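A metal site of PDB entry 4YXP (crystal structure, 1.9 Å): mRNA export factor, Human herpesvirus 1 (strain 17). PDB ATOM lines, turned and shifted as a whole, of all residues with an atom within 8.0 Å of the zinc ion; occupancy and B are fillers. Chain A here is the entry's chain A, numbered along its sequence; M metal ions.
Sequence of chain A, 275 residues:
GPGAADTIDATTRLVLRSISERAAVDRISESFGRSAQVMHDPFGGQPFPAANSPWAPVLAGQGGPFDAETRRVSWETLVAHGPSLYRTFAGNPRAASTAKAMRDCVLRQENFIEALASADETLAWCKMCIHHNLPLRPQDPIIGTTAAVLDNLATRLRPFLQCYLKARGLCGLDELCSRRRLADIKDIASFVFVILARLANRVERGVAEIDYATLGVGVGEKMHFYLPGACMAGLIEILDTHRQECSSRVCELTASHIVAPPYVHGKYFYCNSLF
Four residues have an atom within 4 Å of the zinc ion: Cys 163, His 242, Cys 246 and Cys 251.
N of Cys 251 lies within hydrogen-bond range of OG of Ser 248, 3.1 Å away. The side-chain sulfur (SG) of Cys 246 sits close to the backbone NH (N) of Ser 248 (3.5 Å). ND1 of His 242 sits at hydrogen-bond distance from OE2 of Glu 245, at 3.0 Å.
The zinc ion is bound by NE2 of His 242 (2.1 Å). The zinc ion is bound by the side-chain sulfur (SG) of Cys 163 (2.3 Å). SG of Cys 251 binds the zinc ion. SG of Cys 246 binds the zinc ion, at 2.3 Å.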
ATOM      1  N   PRO A 159      -7.503 -21.745  -4.345  1.00  0.00           N
ATOM      2  CA  PRO A 159      -8.713 -21.133  -4.925  1.00  0.00           C
ATOM      3  C   PRO A 159      -8.426 -19.981  -5.892  1.00  0.00           C
ATOM      4  O   PRO A 159      -9.050 -19.878  -6.945  1.00  0.00           O
ATOM      5  CB  PRO A 159      -9.461 -20.627  -3.692  1.00  0.00           C
ATOM      6  CG  PRO A 159      -9.001 -21.474  -2.583  1.00  0.00           C
ATOM      7  CD  PRO A 159      -7.570 -21.786  -2.873  1.00  0.00           C
ATOM      8  N   PHE A 160      -7.485 -19.128  -5.519  1.00  0.00           N
ATOM      9  CA  PHE A 160      -7.095 -18.010  -6.372  1.00  0.00           C
ATOM     10  C   PHE A 160      -6.466 -18.485  -7.681  1.00  0.00           C
ATOM     11  O   PHE A 160      -6.767 -17.975  -8.760  1.00  0.00           O
ATOM     12  CB  PHE A 160      -6.117 -17.087  -5.632  1.00  0.00           C
ATOM     13  CG  PHE A 160      -5.516 -16.030  -6.502  1.00  0.00           C
ATOM     14  CD1 PHE A 160      -6.265 -14.935  -6.896  1.00  0.00           C
ATOM     15  CD2 PHE A 160      -4.202 -16.131  -6.915  1.00  0.00           C
ATOM     16  CE1 PHE A 160      -5.709 -13.946  -7.696  1.00  0.00           C
ATOM     17  CE2 PHE A 160      -3.640 -15.151  -7.723  1.00  0.00           C
ATOM     18  CZ  PHE A 160      -4.399 -14.061  -8.109  1.00  0.00           C
ATOM     19  N   LEU A 161      -5.594 -19.481  -7.588  1.00  0.00           N
ATOM     20  CA  LEU A 161      -4.875 -19.966  -8.759  1.00  0.00           C
ATOM     21  C   LEU A 161      -5.775 -20.714  -9.729  1.00  0.00           C
ATOM     22  O   LEU A 161      -5.474 -20.784 -10.914  1.00  0.00           O
ATOM     23  CB  LEU A 161      -3.697 -20.856  -8.343  1.00  0.00           C
ATOM     24  CG  LEU A 161      -2.533 -20.133  -7.661  1.00  0.00           C
ATOM     25  CD1 LEU A 161      -1.432 -21.115  -7.286  1.00  0.00           C
ATOM     26  CD2 LEU A 161      -1.963 -19.025  -8.539  1.00  0.00           C
ATOM     27  N   GLN A 162      -6.881 -21.272  -9.246  1.00  0.00           N
ATOM     28  CA  GLN A 162      -7.801 -21.964 -10.148  1.00  0.00           C
ATOM     29  C   GLN A 162      -8.299 -20.985 -11.214  1.00  0.00           C
ATOM     30  O   GLN A 162      -8.391 -21.346 -12.392  1.00  0.00           O
ATOM     31  CB  GLN A 162      -8.991 -22.564  -9.390  1.00  0.00           C
ATOM     32  CG  GLN A 162      -9.801 -23.532 -10.261  1.00  0.00           C
ATOM     33  CD  GLN A 162     -11.015 -24.114  -9.556  1.00  0.00           C
ATOM     34  OE1 GLN A 162     -11.304 -23.772  -8.412  1.00  0.00           O
ATOM     35  NE2 GLN A 162     -11.728 -24.992 -10.247  1.00  0.00           N
ATOM     36  N   CYS A 163      -8.605 -19.755 -10.812  1.00  0.00           N
ATOM     37  CA  CYS A 163      -9.051 -18.727 -11.742  1.00  0.00           C
ATOM     38  C   CYS A 163      -7.869 -18.111 -12.499  1.00  0.00           C
ATOM     39  O   CYS A 163      -7.887 -18.011 -13.723  1.00  0.00           O
ATOM     40  CB  CYS A 163      -9.832 -17.628 -10.997  1.00  0.00           C
ATOM     41  SG  CYS A 163     -10.598 -16.360 -12.065  1.00  0.00           S
ATOM     42  N   TYR A 164      -6.838 -17.712 -11.752  1.00  0.00           N
ATOM     43  CA  TYR A 164      -5.704 -17.004 -12.337  1.00  0.00           C
ATOM     44  C   TYR A 164      -5.005 -17.823 -13.431  1.00  0.00           C
ATOM     45  O   TYR A 164      -4.716 -17.302 -14.514  1.00  0.00           O
ATOM     46  CB  TYR A 164      -4.693 -16.625 -11.259  1.00  0.00           C
ATOM     47  CG  TYR A 164      -3.379 -16.076 -11.793  1.00  0.00           C
ATOM     48  CD1 TYR A 164      -3.241 -14.722 -12.093  1.00  0.00           C
ATOM     49  CD2 TYR A 164      -2.283 -16.901 -11.979  1.00  0.00           C
ATOM     50  CE1 TYR A 164      -2.045 -14.220 -12.582  1.00  0.00           C
ATOM     51  CE2 TYR A 164      -1.089 -16.413 -12.467  1.00  0.00           C
ATOM     52  CZ  TYR A 164      -0.974 -15.068 -12.765  1.00  0.00           C
ATOM     53  OH  TYR A 164       0.222 -14.574 -13.247  1.00  0.00           O
ATOM     54  N   LEU A 165      -4.723 -19.087 -13.152  1.00  0.00           N
ATOM     55  CA  LEU A 165      -4.000 -19.930 -14.115  1.00  0.00           C
ATOM     56  C   LEU A 165      -4.839 -20.154 -15.379  1.00  0.00           C
ATOM     57  O   LEU A 165      -4.282 -20.299 -16.466  1.00  0.00           O
ATOM     58  CB  LEU A 165      -3.601 -21.264 -13.489  1.00  0.00           C
ATOM     59  CG  LEU A 165      -2.550 -21.197 -12.379  1.00  0.00           C
ATOM     60  CD1 LEU A 165      -2.349 -22.561 -11.726  1.00  0.00           C
ATOM     61  CD2 LEU A 165      -1.219 -20.667 -12.915  1.00  0.00           C
ATOM     62  N   LYS A 166      -6.156 -20.173 -15.238  1.00  0.00           N
ATOM     63  CA  LYS A 166      -7.037 -20.277 -16.401  1.00  0.00           C
ATOM     64  C   LYS A 166      -6.894 -19.042 -17.282  1.00  0.00           C
ATOM     65  O   LYS A 166      -6.824 -19.149 -18.508  1.00  0.00           O
ATOM     66  CB  LYS A 166      -8.503 -20.454 -15.977  1.00  0.00           C
ATOM     67  CG  LYS A 166      -8.996 -21.890 -16.021  1.00  0.00           C
ATOM     68  CD  LYS A 166     -10.489 -21.976 -15.706  1.00  0.00           C
ATOM     69  CE  LYS A 166     -10.934 -23.418 -15.471  1.00  0.00           C
ATOM     70  NZ  LYS A 166     -10.378 -23.979 -14.199  1.00  0.00           N
ATOM     71  N   ALA A 167      -6.860 -17.867 -16.657  1.00  0.00           N
ATOM     72  CA  ALA A 167      -6.714 -16.616 -17.396  1.00  0.00           C
ATOM     73  C   ALA A 167      -5.395 -16.557 -18.158  1.00  0.00           C
ATOM     74  O   ALA A 167      -5.317 -15.963 -19.239  1.00  0.00           O
ATOM     75  CB  ALA A 167      -6.816 -15.428 -16.444  1.00  0.00           C
ATOM     76  N   HIS A 242      -4.534  -9.107 -10.800  1.00  0.00           N
ATOM     77  CA  HIS A 242      -5.425 -10.034 -11.509  1.00  0.00           C
ATOM     78  C   HIS A 242      -6.856  -9.481 -11.587  1.00  0.00           C
ATOM     79  O   HIS A 242      -7.577  -9.740 -12.553  1.00  0.00           O
ATOM     80  CB  HIS A 242      -5.430 -11.410 -10.827  1.00  0.00           C
ATOM     81  CG  HIS A 242      -6.501 -12.339 -11.340  1.00  0.00           C
ATOM     82  ND1 HIS A 242      -6.542 -12.763 -12.647  1.00  0.00           N
ATOM     83  CD2 HIS A 242      -7.549 -12.913 -10.716  1.00  0.00           C
ATOM     84  CE1 HIS A 242      -7.588 -13.568 -12.812  1.00  0.00           C
ATOM     85  NE2 HIS A 242      -8.211 -13.676 -11.655  1.00  0.00           N
ATOM     86  N   ARG A 243      -7.257  -8.699 -10.592  1.00  0.00           N
ATOM     87  CA  ARG A 243      -8.607  -8.127 -10.573  1.00  0.00           C
ATOM     88  C   ARG A 243      -8.852  -7.123 -11.711  1.00  0.00           C
ATOM     89  O   ARG A 243      -9.997  -6.751 -11.974  1.00  0.00           O
ATOM     90  CB  ARG A 243      -8.879  -7.460  -9.220  1.00  0.00           C
ATOM     91  CG  ARG A 243      -8.050  -6.202  -8.947  1.00  0.00           C
ATOM     92  CD  ARG A 243      -8.099  -5.827  -7.471  1.00  0.00           C
ATOM     93  NE  ARG A 243      -7.382  -6.792  -6.628  1.00  0.00           N
ATOM     94  CZ  ARG A 243      -7.486  -6.856  -5.308  1.00  0.00           C
ATOM     95  NH1 ARG A 243      -8.297  -6.028  -4.647  1.00  0.00           N
ATOM     96  NH2 ARG A 243      -6.801  -7.767  -4.623  1.00  0.00           N
ATOM     97  N   GLU A 245      -8.339  -7.790 -14.776  1.00  0.00           N
ATOM     98  CA  GLU A 245      -8.701  -8.592 -15.944  1.00  0.00           C
ATOM     99  C   GLU A 245      -9.823  -9.583 -15.636  1.00  0.00           C
ATOM    100  O   GLU A 245     -10.317 -10.265 -16.540  1.00  0.00           O
ATOM    101  CB  GLU A 245      -7.462  -9.351 -16.463  1.00  0.00           C
ATOM    102  CG  GLU A 245      -6.960 -10.427 -15.505  1.00  0.00           C
ATOM    103  CD  GLU A 245      -5.703 -11.125 -15.991  1.00  0.00           C
ATOM    104  OE1 GLU A 245      -5.224 -10.805 -17.103  1.00  0.00           O
ATOM    105  OE2 GLU A 245      -5.173 -11.979 -15.248  1.00  0.00           O
ATOM    106  N   CYS A 246     -10.224  -9.650 -14.367  1.00  0.00           N
ATOM    107  CA  CYS A 246     -11.191 -10.649 -13.903  1.00  0.00           C
ATOM    108  C   CYS A 246     -12.456  -9.985 -13.352  1.00  0.00           C
ATOM    109  O   CYS A 246     -12.380  -9.084 -12.529  1.00  0.00           O
ATOM    110  CB  CYS A 246     -10.539 -11.539 -12.835  1.00  0.00           C
ATOM    111  SG  CYS A 246     -11.604 -12.847 -12.147  1.00  0.00           S
ATOM    112  N   SER A 247     -13.606 -10.462 -13.805  1.00  0.00           N
ATOM    113  CA  SER A 247     -14.890  -9.876 -13.417  1.00  0.00           C
ATOM    114  C   SER A 247     -15.572 -10.629 -12.268  1.00  0.00           C
ATOM    115  O   SER A 247     -16.693 -10.288 -11.885  1.00  0.00           O
ATOM    116  CB  SER A 247     -15.840  -9.843 -14.619  1.00  0.00           C
ATOM    117  OG  SER A 247     -16.126 -11.149 -15.068  1.00  0.00           O
ATOM    118  N   SER A 248     -14.903 -11.625 -11.712  1.00  0.00           N
ATOM    119  CA  SER A 248     -15.474 -12.410 -10.614  1.00  0.00           C
ATOM    120  C   SER A 248     -15.298 -11.724  -9.265  1.00  0.00           C
ATOM    121  O   SER A 248     -14.173 -11.503  -8.813  1.00  0.00           O
ATOM    122  CB  SER A 248     -14.830 -13.806 -10.566  1.00  0.00           C
ATOM    123  OG  SER A 248     -15.204 -14.495  -9.388  1.00  0.00           O
ATOM    124  N   ARG A 249     -16.416 -11.394  -8.626  1.00  0.00           N
ATOM    125  CA  ARG A 249     -16.390 -10.770  -7.293  1.00  0.00           C
ATOM    126  C   ARG A 249     -15.845 -11.752  -6.254  1.00  0.00           C
ATOM    127  O   ARG A 249     -15.112 -11.353  -5.345  1.00  0.00           O
ATOM    128  CB  ARG A 249     -17.790 -10.289  -6.905  1.00  0.00           C
ATOM    129  CG  ARG A 249     -17.939  -9.836  -5.457  1.00  0.00           C
ATOM    130  CD  ARG A 249     -17.108  -8.598  -5.135  1.00  0.00           C
ATOM    131  NE  ARG A 249     -17.388  -8.104  -3.796  1.00  0.00           N
ATOM    132  CZ  ARG A 249     -16.846  -7.011  -3.257  1.00  0.00           C
ATOM    133  NH1 ARG A 249     -15.991  -6.280  -3.953  1.00  0.00           N
ATOM    134  NH2 ARG A 249     -17.171  -6.653  -2.029  1.00  0.00           N
ATOM    135  N   VAL A 250     -16.220 -13.019  -6.376  1.00  0.00           N
ATOM    136  CA  VAL A 250     -15.699 -14.050  -5.500  1.00  0.00           C
ATOM    137  C   VAL A 250     -14.174 -14.068  -5.577  1.00  0.00           C
ATOM    138  O   VAL A 250     -13.493 -14.169  -4.560  1.00  0.00           O
ATOM    139  CB  VAL A 250     -16.289 -15.434  -5.864  1.00  0.00           C
ATOM    140  CG1 VAL A 250     -15.490 -16.564  -5.206  1.00  0.00           C
ATOM    141  CG2 VAL A 250     -17.751 -15.503  -5.432  1.00  0.00           C
ATOM    142  N   CYS A 251     -13.642 -13.956  -6.793  1.00  0.00           N
ATOM    143  CA  CYS A 251     -12.198 -13.980  -6.995  1.00  0.00           C
ATOM    144  C   CYS A 251     -11.541 -12.751  -6.356  1.00  0.00           C
ATOM    145  O   CYS A 251     -10.502 -12.856  -5.725  1.00  0.00           O
ATOM    146  CB  CYS A 251     -11.859 -14.056  -8.479  1.00  0.00           C
ATOM    147  SG  CYS A 251     -10.075 -14.220  -8.838  1.00  0.00           S
ATOM    148  N   GLU A 252     -12.158 -11.580  -6.525  1.00  0.00           N
ATOM    149  CA  GLU A 252     -11.612 -10.349  -5.949  1.00  0.00           C
ATOM    150  C   GLU A 252     -11.635 -10.414  -4.426  1.00  0.00           C
ATOM    151  O   GLU A 252     -10.713  -9.928  -3.770  1.00  0.00           O
ATOM    152  CB  GLU A 252     -12.396  -9.118  -6.437  1.00  0.00           C
ATOM    153  CG  GLU A 252     -11.727  -7.795  -6.084  1.00  0.00           C
ATOM    154  CD  GLU A 252     -12.504  -6.580  -6.572  1.00  0.00           C
ATOM    155  OE1 GLU A 252     -13.680  -6.739  -6.967  1.00  0.00           O
ATOM    156  OE2 GLU A 252     -11.940  -5.471  -6.550  1.00  0.00           O
ATOM    157  N   THR A 254     -11.439 -13.241  -2.657  1.00  0.00           N
ATOM    158  CA  THR A 254     -10.437 -14.231  -2.311  1.00  0.00           C
ATOM    159  C   THR A 254      -9.027 -13.630  -2.322  1.00  0.00           C
ATOM    160  O   THR A 254      -8.265 -13.793  -1.373  1.00  0.00           O
ATOM    161  CB  THR A 254     -10.495 -15.435  -3.276  1.00  0.00           C
ATOM    162  OG1 THR A 254     -11.784 -16.047  -3.197  1.00  0.00           O
ATOM    163  CG2 THR A 254      -9.412 -16.473  -2.942  1.00  0.00           C
ATOM    164  N   ALA A 255      -8.692 -12.946  -3.409  1.00  0.00           N
ATOM    165  CA  ALA A 255      -7.395 -12.308  -3.546  1.00  0.00           C
ATOM    166  C   ALA A 255      -7.188 -11.279  -2.432  1.00  0.00           C
ATOM    167  O   ALA A 255      -6.139 -11.240  -1.800  1.00  0.00           O
ATOM    168  CB  ALA A 255      -7.262 -11.650  -4.912  1.00  0.00           C
HETATM  169 ZN    ZN M   1     -10.096 -14.355 -11.165  1.00  0.00          ZN
